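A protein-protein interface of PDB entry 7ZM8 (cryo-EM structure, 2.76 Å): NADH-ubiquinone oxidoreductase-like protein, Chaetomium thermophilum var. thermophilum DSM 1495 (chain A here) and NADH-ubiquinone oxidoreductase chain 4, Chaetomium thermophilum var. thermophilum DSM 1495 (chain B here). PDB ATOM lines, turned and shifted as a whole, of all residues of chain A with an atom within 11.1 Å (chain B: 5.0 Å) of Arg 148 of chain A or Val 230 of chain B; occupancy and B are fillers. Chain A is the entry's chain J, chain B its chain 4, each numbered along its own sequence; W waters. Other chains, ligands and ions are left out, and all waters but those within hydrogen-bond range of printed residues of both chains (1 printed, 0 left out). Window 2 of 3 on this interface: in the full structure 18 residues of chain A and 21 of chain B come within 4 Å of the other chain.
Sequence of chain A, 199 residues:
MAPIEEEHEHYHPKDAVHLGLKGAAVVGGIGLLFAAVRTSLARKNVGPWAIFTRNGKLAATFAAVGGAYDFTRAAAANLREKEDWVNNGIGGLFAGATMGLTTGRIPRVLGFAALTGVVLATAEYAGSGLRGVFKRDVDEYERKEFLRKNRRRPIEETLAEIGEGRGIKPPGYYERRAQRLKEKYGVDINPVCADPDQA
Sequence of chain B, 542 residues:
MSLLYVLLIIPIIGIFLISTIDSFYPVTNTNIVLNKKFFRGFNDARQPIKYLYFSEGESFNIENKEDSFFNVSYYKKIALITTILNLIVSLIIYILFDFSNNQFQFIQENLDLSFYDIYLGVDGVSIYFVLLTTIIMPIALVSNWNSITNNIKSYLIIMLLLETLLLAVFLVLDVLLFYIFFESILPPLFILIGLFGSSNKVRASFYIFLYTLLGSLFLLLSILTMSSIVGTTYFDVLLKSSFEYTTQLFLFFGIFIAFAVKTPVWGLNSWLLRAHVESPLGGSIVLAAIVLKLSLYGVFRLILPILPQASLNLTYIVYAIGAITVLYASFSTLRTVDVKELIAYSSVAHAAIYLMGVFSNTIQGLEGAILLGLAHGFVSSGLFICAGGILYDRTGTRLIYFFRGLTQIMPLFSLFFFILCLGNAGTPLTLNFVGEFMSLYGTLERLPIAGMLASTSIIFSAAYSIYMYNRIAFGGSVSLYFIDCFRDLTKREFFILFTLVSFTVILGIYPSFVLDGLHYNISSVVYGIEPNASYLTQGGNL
Printed residues of chain B within 4 Å of Lys 144 of chain A: Ser 228 (3.2 Å) and Ile 229 (3.4 Å).
Printed residues of chain B within 4 Å of Leu 147 of chain A: Ile 229 (3.8 Å).
Arg 151 of chain A touches none of the printed residues of chain B.
Of the printed residues of chain B, Arg 153 of chain A touches Phe 243 (3.5 Å).
Met 226 of chain B touches none of the printed residues of chain A.
Ser 228 of chain B touches one residue of chain A.
Ile 229 of chain B touches just these residues of chain A: Lys 144 (3.4 Å), Leu 147 (3.8 Å) and Arg 148 (3.8 Å).
No residue of chain A comes within 4 Å of Gly 231 of chain B.
No residue of chain A comes within 4 Å of Thr 232 of chain B.
No residue of chain A comes within 4 Å of Val 237 of chain B.
Ser 241 of chain B touches just one residue of chain A: Arg 148.
Of the printed residues of chain A, Phe 243 of chain B touches Arg 153 (3.5 Å).
NH1 of Arg 153 of chain A sits at hydrogen-bond distance from O of Phe 243 of chain B (3.5 Å).
O of Ser 228 of chain B sits close to NZ of Lys 144 of chain A (3.5 Å).
Water W1 lies within hydrogen-bond range of O of Phe 243 of chain B (2.6 Å) and NH1 of Arg 153 of chain A (3.0 Å).
Hydrophobic or aromatic side chains of chain A that line the printed part of chain B: Leu 147.
Among the printed residues, 7 pairs touch across the chains.
Among the printed residues, merely in contact across the chains: Lys 144 of chain A with Ile 229 of chain B, Leu 147 of chain A with Ile 229 of chain B, Arg 148 of chain A with Ile 229 of chain B, Arg 148 of chain A with Val 230 of chain B and Arg 148 of chain A with Ser 241 of chain B.
The backbone carbonyl oxygen (O) of Val 237 of chain B lies within hydrogen-bond range of the side-chain hydroxyl (OG) of Ser 241 of chain B, at 3.1 Å.
The guanidinium group of Arg 151 of chain A is in hydrogen-bond range of the backbone carbonyl oxygen of Arg 148 of chain A, 3.4 Å away.
ND2 of Asn 150 of chain A sits close to NH2 of Arg 153 of chain A (3.3 Å).
The side-chain carboxylate of Glu 145 of chain A is in salt-bridge range of the guanidinium group of Arg 148 of chain A, 2.9 Å away.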
ATOM      1  N   GLU A 140      39.148  21.226  -3.059  1.00  0.00           N
ATOM      2  CA  GLU A 140      38.144  21.342  -4.147  1.00  0.00           C
ATOM      3  C   GLU A 140      36.861  20.602  -3.784  1.00  0.00           C
ATOM      4  O   GLU A 140      35.801  21.122  -4.092  1.00  0.00           O
ATOM      5  CB  GLU A 140      38.723  20.881  -5.483  1.00  0.00           C
ATOM      6  CG  GLU A 140      39.397  21.998  -6.256  1.00  0.00           C
ATOM      7  CD  GLU A 140      38.470  23.123  -6.690  1.00  0.00           C
ATOM      8  OE1 GLU A 140      37.270  22.856  -6.895  1.00  0.00           O
ATOM      9  OE2 GLU A 140      38.952  24.266  -6.817  1.00  0.00           O
ATOM     10  N   TYR A 141      36.973  19.437  -3.158  1.00  0.00           N
ATOM     11  CA  TYR A 141      35.780  18.632  -2.799  1.00  0.00           C
ATOM     12  C   TYR A 141      34.928  19.395  -1.799  1.00  0.00           C
ATOM     13  O   TYR A 141      33.711  19.449  -1.971  1.00  0.00           O
ATOM     14  CB  TYR A 141      36.201  17.279  -2.237  1.00  0.00           C
ATOM     15  CG  TYR A 141      35.087  16.352  -1.839  1.00  0.00           C
ATOM     16  CD1 TYR A 141      34.427  15.582  -2.779  1.00  0.00           C
ATOM     17  CD2 TYR A 141      34.709  16.233  -0.516  1.00  0.00           C
ATOM     18  CE1 TYR A 141      33.407  14.723  -2.414  1.00  0.00           C
ATOM     19  CE2 TYR A 141      33.699  15.372  -0.131  1.00  0.00           C
ATOM     20  CZ  TYR A 141      33.047  14.617  -1.085  1.00  0.00           C
ATOM     21  OH  TYR A 141      32.052  13.773  -0.703  1.00  0.00           O
ATOM     22  N   GLU A 142      35.569  20.007  -0.812  1.00  0.00           N
ATOM     23  CA  GLU A 142      34.829  20.817   0.181  1.00  0.00           C
ATOM     24  C   GLU A 142      34.181  22.011  -0.524  1.00  0.00           C
ATOM     25  O   GLU A 142      33.008  22.284  -0.237  1.00  0.00           O
ATOM     26  CB  GLU A 142      35.781  21.231   1.301  1.00  0.00           C
ATOM     27  CG  GLU A 142      35.078  21.811   2.513  1.00  0.00           C
ATOM     28  CD  GLU A 142      34.238  20.819   3.300  1.00  0.00           C
ATOM     29  OE1 GLU A 142      34.596  19.625   3.323  1.00  0.00           O
ATOM     30  OE2 GLU A 142      33.223  21.244   3.885  1.00  0.00           O
ATOM     31  N   ARG A 143      34.910  22.682  -1.416  1.00  0.00           N
ATOM     32  CA  ARG A 143      34.385  23.906  -2.077  1.00  0.00           C
ATOM     33  C   ARG A 143      33.188  23.568  -2.960  1.00  0.00           C
ATOM     34  O   ARG A 143      32.187  24.287  -2.886  1.00  0.00           O
ATOM     35  CB  ARG A 143      35.489  24.549  -2.914  1.00  0.00           C
ATOM     36  CG  ARG A 143      35.053  25.792  -3.675  1.00  0.00           C
ATOM     37  CD  ARG A 143      35.838  25.982  -4.958  1.00  0.00           C
ATOM     38  NE  ARG A 143      35.424  27.184  -5.667  1.00  0.00           N
ATOM     39  CZ  ARG A 143      36.007  28.370  -5.541  1.00  0.00           C
ATOM     40  NH1 ARG A 143      35.554  29.406  -6.225  1.00  0.00           N
ATOM     41  NH2 ARG A 143      37.043  28.517  -4.735  1.00  0.00           N
ATOM     42  N   LYS A 144      33.296  22.498  -3.750  1.00  0.00           N
ATOM     43  CA  LYS A 144      32.223  22.104  -4.693  1.00  0.00           C
ATOM     44  C   LYS A 144      31.018  21.617  -3.909  1.00  0.00           C
ATOM     45  O   LYS A 144      29.894  21.978  -4.269  1.00  0.00           O
ATOM     46  CB  LYS A 144      32.767  21.067  -5.677  1.00  0.00           C
ATOM     47  CG  LYS A 144      33.881  21.545  -6.595  1.00  0.00           C
ATOM     48  CD  LYS A 144      33.534  22.801  -7.360  1.00  0.00           C
ATOM     49  CE  LYS A 144      32.410  22.606  -8.353  1.00  0.00           C
ATOM     50  NZ  LYS A 144      32.049  23.878  -9.023  1.00  0.00           N
ATOM     51  N   GLU A 145      31.263  20.822  -2.875  1.00  0.00           N
ATOM     52  CA  GLU A 145      30.157  20.240  -2.075  1.00  0.00           C
ATOM     53  C   GLU A 145      29.405  21.337  -1.315  1.00  0.00           C
ATOM     54  O   GLU A 145      28.180  21.238  -1.215  1.00  0.00           O
ATOM     55  CB  GLU A 145      30.671  19.063  -1.248  1.00  0.00           C
ATOM     56  CG  GLU A 145      30.915  17.812  -2.064  1.00  0.00           C
ATOM     57  CD  GLU A 145      29.672  16.996  -2.365  1.00  0.00           C
ATOM     58  OE1 GLU A 145      29.242  16.246  -1.478  1.00  0.00           O
ATOM     59  OE2 GLU A 145      29.140  17.115  -3.481  1.00  0.00           O
ATOM     60  N   PHE A 146      30.103  22.357  -0.828  1.00  0.00           N
ATOM     61  CA  PHE A 146      29.452  23.477  -0.112  1.00  0.00           C
ATOM     62  C   PHE A 146      28.517  24.187  -1.064  1.00  0.00           C
ATOM     63  O   PHE A 146      27.427  24.582  -0.663  1.00  0.00           O
ATOM     64  CB  PHE A 146      30.480  24.519   0.321  1.00  0.00           C
ATOM     65  CG  PHE A 146      29.875  25.721   0.998  1.00  0.00           C
ATOM     66  CD1 PHE A 146      29.341  25.622   2.271  1.00  0.00           C
ATOM     67  CD2 PHE A 146      29.821  26.946   0.355  1.00  0.00           C
ATOM     68  CE1 PHE A 146      28.770  26.723   2.886  1.00  0.00           C
ATOM     69  CE2 PHE A 146      29.245  28.044   0.969  1.00  0.00           C
ATOM     70  CZ  PHE A 146      28.725  27.932   2.235  1.00  0.00           C
ATOM     71  N   LEU A 147      28.964  24.356  -2.295  1.00  0.00           N
ATOM     72  CA  LEU A 147      28.152  25.061  -3.296  1.00  0.00           C
ATOM     73  C   LEU A 147      26.899  24.253  -3.609  1.00  0.00           C
ATOM     74  O   LEU A 147      25.864  24.877  -3.802  1.00  0.00           O
ATOM     75  CB  LEU A 147      29.040  25.293  -4.510  1.00  0.00           C
ATOM     76  CG  LEU A 147      30.111  26.366  -4.355  1.00  0.00           C
ATOM     77  CD1 LEU A 147      30.980  26.426  -5.601  1.00  0.00           C
ATOM     78  CD2 LEU A 147      29.481  27.718  -4.074  1.00  0.00           C
ATOM     79  N   ARG A 148      26.980  22.924  -3.633  1.00  0.00           N
ATOM     80  CA  ARG A 148      25.826  22.070  -4.025  1.00  0.00           C
ATOM     81  C   ARG A 148      24.844  21.919  -2.858  1.00  0.00           C
ATOM     82  O   ARG A 148      23.641  21.788  -3.115  1.00  0.00           O
ATOM     83  CB  ARG A 148      26.324  20.677  -4.421  1.00  0.00           C
ATOM     84  CG  ARG A 148      25.211  19.687  -4.739  1.00  0.00           C
ATOM     85  CD  ARG A 148      25.663  18.267  -5.012  1.00  0.00           C
ATOM     86  NE  ARG A 148      26.315  17.633  -3.882  1.00  0.00           N
ATOM     87  CZ  ARG A 148      25.746  16.743  -3.088  1.00  0.00           C
ATOM     88  NH1 ARG A 148      26.428  16.226  -2.085  1.00  0.00           N
ATOM     89  NH2 ARG A 148      24.503  16.358  -3.305  1.00  0.00           N
ATOM     90  N   LYS A 149      25.328  21.971  -1.624  1.00  0.00           N
ATOM     91  CA  LYS A 149      24.469  21.783  -0.466  1.00  0.00           C
ATOM     92  C   LYS A 149      24.156  23.079   0.269  1.00  0.00           C
ATOM     93  O   LYS A 149      23.529  23.037   1.330  1.00  0.00           O
ATOM     94  CB  LYS A 149      25.100  20.768   0.483  1.00  0.00           C
ATOM     95  CG  LYS A 149      25.026  19.350  -0.042  1.00  0.00           C
ATOM     96  CD  LYS A 149      25.847  18.403   0.803  1.00  0.00           C
ATOM     97  CE  LYS A 149      27.324  18.534   0.496  1.00  0.00           C
ATOM     98  NZ  LYS A 149      28.142  17.566   1.270  1.00  0.00           N
ATOM     99  N   ASN A 150      24.559  24.228  -0.271  1.00  0.00           N
ATOM    100  CA  ASN A 150      24.192  25.524   0.306  1.00  0.00           C
ATOM    101  C   ASN A 150      22.826  25.939  -0.234  1.00  0.00           C
ATOM    102  O   ASN A 150      22.666  26.918  -0.960  1.00  0.00           O
ATOM    103  CB  ASN A 150      25.257  26.567   0.000  1.00  0.00           C
ATOM    104  CG  ASN A 150      24.989  27.886   0.679  1.00  0.00           C
ATOM    105  OD1 ASN A 150      24.326  27.939   1.713  1.00  0.00           O
ATOM    106  ND2 ASN A 150      25.503  28.964   0.102  1.00  0.00           N
ATOM    107  N   ARG A 151      21.824  25.150   0.139  1.00  0.00           N
ATOM    108  CA  ARG A 151      20.496  25.307  -0.435  1.00  0.00           C
ATOM    109  C   ARG A 151      19.748  26.495   0.157  1.00  0.00           C
ATOM    110  O   ARG A 151      19.015  27.181  -0.559  1.00  0.00           O
ATOM    111  CB  ARG A 151      19.710  24.012  -0.253  1.00  0.00           C
ATOM    112  CG  ARG A 151      20.488  22.796  -0.678  1.00  0.00           C
ATOM    113  CD  ARG A 151      19.649  21.862  -1.523  1.00  0.00           C
ATOM    114  NE  ARG A 151      20.459  20.881  -2.243  1.00  0.00           N
ATOM    115  CZ  ARG A 151      20.919  19.752  -1.714  1.00  0.00           C
ATOM    116  NH1 ARG A 151      21.642  18.923  -2.449  1.00  0.00           N
ATOM    117  NH2 ARG A 151      20.669  19.453  -0.452  1.00  0.00           N
ATOM    118  N   ARG A 152      19.800  26.685   1.472  1.00  0.00           N
ATOM    119  CA  ARG A 152      19.108  27.878   2.012  1.00  0.00           C
ATOM    120  C   ARG A 152      20.135  28.871   2.508  1.00  0.00           C
ATOM    121  O   ARG A 152      21.217  28.435   2.914  1.00  0.00           O
ATOM    122  CB  ARG A 152      18.154  27.590   3.166  1.00  0.00           C
ATOM    123  CG  ARG A 152      17.228  26.403   3.004  1.00  0.00           C
ATOM    124  CD  ARG A 152      16.362  26.371   4.249  1.00  0.00           C
ATOM    125  NE  ARG A 152      15.248  27.305   4.227  1.00  0.00           N
ATOM    126  CZ  ARG A 152      14.356  27.418   5.200  1.00  0.00           C
ATOM    127  NH1 ARG A 152      14.458  26.659   6.276  1.00  0.00           N
ATOM    128  NH2 ARG A 152      13.367  28.287   5.104  1.00  0.00           N
ATOM    129  N   ARG A 153      19.766  30.146   2.533  1.00  0.00           N
ATOM    130  CA  ARG A 153      20.704  31.210   2.947  1.00  0.00           C
ATOM    131  C   ARG A 153      20.022  32.104   3.962  1.00  0.00           C
ATOM    132  O   ARG A 153      18.809  32.056   4.050  1.00  0.00           O
ATOM    133  CB  ARG A 153      21.132  32.033   1.728  1.00  0.00           C
ATOM    134  CG  ARG A 153      22.258  31.424   0.908  1.00  0.00           C
ATOM    135  CD  ARG A 153      22.512  32.284  -0.311  1.00  0.00           C
ATOM    136  NE  ARG A 153      23.687  31.897  -1.077  1.00  0.00           N
ATOM    137  CZ  ARG A 153      23.692  30.979  -2.033  1.00  0.00           C
ATOM    138  NH1 ARG A 153      22.582  30.334  -2.338  1.00  0.00           N
ATOM    139  NH2 ARG A 153      24.811  30.696  -2.669  1.00  0.00           N
ATOM    140  N   MET B 226      26.723  25.205 -14.410  1.00  0.00           N
ATOM    141  CA  MET B 226      25.755  24.755 -13.388  1.00  0.00           C
ATOM    142  C   MET B 226      25.978  23.275 -13.084  1.00  0.00           C
ATOM    143  O   MET B 226      25.869  22.908 -11.916  1.00  0.00           O
ATOM    144  CB  MET B 226      24.316  24.922 -13.870  1.00  0.00           C
ATOM    145  CG  MET B 226      23.933  26.314 -14.223  1.00  0.00           C
ATOM    146  SD  MET B 226      22.253  26.278 -14.844  1.00  0.00           S
ATOM    147  CE  MET B 226      22.113  27.954 -15.459  1.00  0.00           C
ATOM    148  N   SER B 227      26.259  22.464 -14.102  1.00  0.00           N
ATOM    149  CA  SER B 227      26.484  21.014 -13.924  1.00  0.00           C
ATOM    150  C   SER B 227      27.748  20.803 -13.106  1.00  0.00           C
ATOM    151  O   SER B 227      27.773  19.877 -12.310  1.00  0.00           O
ATOM    152  CB  SER B 227      26.603  20.374 -15.253  1.00  0.00           C
ATOM    153  OG  SER B 227      26.659  18.962 -15.131  1.00  0.00           O
ATOM    154  N   SER B 228      28.761  21.631 -13.322  1.00  0.00           N
ATOM    155  CA  SER B 228      30.038  21.528 -12.580  1.00  0.00           C
ATOM    156  C   SER B 228      29.807  21.829 -11.110  1.00  0.00           C
ATOM    157  O   SER B 228      30.367  21.121 -10.289  1.00  0.00           O
ATOM    158  CB  SER B 228      31.083  22.422 -13.171  1.00  0.00           C
ATOM    159  OG  SER B 228      30.902  23.764 -12.761  1.00  0.00           O
ATOM    160  N   ILE B 229      28.952  22.794 -10.805  1.00  0.00           N
ATOM    161  CA  ILE B 229      28.732  23.245  -9.405  1.00  0.00           C
ATOM    162  C   ILE B 229      27.779  22.285  -8.698  1.00  0.00           C
ATOM    163  O   ILE B 229      27.949  22.078  -7.502  1.00  0.00           O
ATOM    164  CB  ILE B 229      28.182  24.685  -9.439  1.00  0.00           C
ATOM    165  CG1 ILE B 229      29.161  25.646 -10.114  1.00  0.00           C
ATOM    166  CG2 ILE B 229      27.787  25.172  -8.052  1.00  0.00           C
ATOM    167  CD1 ILE B 229      28.663  27.061 -10.210  1.00  0.00           C
ATOM    168  N   VAL B 230      26.838  21.694  -9.416  1.00  0.00           N
ATOM    169  CA  VAL B 230      25.814  20.824  -8.769  1.00  0.00           C
ATOM    170  C   VAL B 230      26.080  19.327  -9.000  1.00  0.00           C
ATOM    171  O   VAL B 230      25.746  18.538  -8.117  1.00  0.00           O
ATOM    172  CB  VAL B 230      24.408  21.255  -9.237  1.00  0.00           C
ATOM    173  CG1 VAL B 230      23.299  20.382  -8.673  1.00  0.00           C
ATOM    174  CG2 VAL B 230      24.131  22.715  -8.933  1.00  0.00           C
ATOM    175  N   GLY B 231      26.677  18.945 -10.124  1.00  0.00           N
ATOM    176  CA  GLY B 231      27.018  17.541 -10.400  1.00  0.00           C
ATOM    177  C   GLY B 231      26.025  16.855 -11.308  1.00  0.00           C
ATOM    178  O   GLY B 231      26.280  15.718 -11.705  1.00  0.00           O
ATOM    179  N   THR B 232      24.930  17.531 -11.628  1.00  0.00           N
ATOM    180  CA  THR B 232      23.954  16.937 -12.564  1.00  0.00           C
ATOM    181  C   THR B 232      23.051  18.055 -13.063  1.00  0.00           C
ATOM    182  O   THR B 232      23.114  19.146 -12.491  1.00  0.00           O
ATOM    183  CB  THR B 232      23.086  15.865 -11.881  1.00  0.00           C
ATOM    184  OG1 THR B 232      22.103  15.383 -12.794  1.00  0.00           O
ATOM    185  CG2 THR B 232      22.395  16.363 -10.632  1.00  0.00           C
ATOM    186  N   VAL B 237      17.124  17.851  -8.956  1.00  0.00           N
ATOM    187  CA  VAL B 237      18.341  18.174  -8.165  1.00  0.00           C
ATOM    188  C   VAL B 237      18.761  19.622  -8.436  1.00  0.00           C
ATOM    189  O   VAL B 237      19.206  20.271  -7.494  1.00  0.00           O
ATOM    190  CB  VAL B 237      19.453  17.152  -8.471  1.00  0.00           C
ATOM    191  CG1 VAL B 237      20.670  17.342  -7.585  1.00  0.00           C
ATOM    192  CG2 VAL B 237      18.940  15.726  -8.386  1.00  0.00           C
ATOM    193  N   LEU B 238      18.596  20.110  -9.670  1.00  0.00           N
ATOM    194  CA  LEU B 238      19.022  21.470  -9.979  1.00  0.00           C
ATOM    195  C   LEU B 238      18.096  22.501  -9.345  1.00  0.00           C
ATOM    196  O   LEU B 238      18.546  23.567  -8.916  1.00  0.00           O
ATOM    197  CB  LEU B 238      19.088  21.653 -11.496  1.00  0.00           C
ATOM    198  CG  LEU B 238      19.617  22.943 -12.126  1.00  0.00           C
ATOM    199  CD1 LEU B 238      20.996  23.326 -11.611  1.00  0.00           C
ATOM    200  CD2 LEU B 238      19.635  22.796 -13.633  1.00  0.00           C
ATOM    201  N   SER B 241      18.866  23.399  -5.742  1.00  0.00           N
ATOM    202  CA  SER B 241      20.116  24.155  -5.539  1.00  0.00           C
ATOM    203  C   SER B 241      19.959  25.666  -5.697  1.00  0.00           C
ATOM    204  O   SER B 241      19.287  26.096  -6.643  1.00  0.00           O
ATOM    205  CB  SER B 241      21.094  23.584  -6.506  1.00  0.00           C
ATOM    206  OG  SER B 241      21.316  22.212  -6.219  1.00  0.00           O
ATOM    207  N   PHE B 243      22.099  29.174  -6.325  1.00  0.00           N
ATOM    208  CA  PHE B 243      23.417  29.687  -6.732  1.00  0.00           C
ATOM    209  C   PHE B 243      23.737  30.996  -6.034  1.00  0.00           C
ATOM    210  O   PHE B 243      22.820  31.653  -5.547  1.00  0.00           O
ATOM    211  CB  PHE B 243      23.454  29.861  -8.247  1.00  0.00           C
ATOM    212  CG  PHE B 243      23.488  28.574  -9.026  1.00  0.00           C
ATOM    213  CD1 PHE B 243      24.691  27.937  -9.287  1.00  0.00           C
ATOM    214  CD2 PHE B 243      22.321  28.001  -9.497  1.00  0.00           C
ATOM    215  CE1 PHE B 243      24.722  26.755 -10.007  1.00  0.00           C
ATOM    216  CE2 PHE B 243      22.354  26.818 -10.213  1.00  0.00           C
ATOM    217  CZ  PHE B 243      23.553  26.197 -10.465  1.00  0.00           C
HETATM  218  O   HOH W   1      21.538  32.851  -3.566  1.00  0.00           O
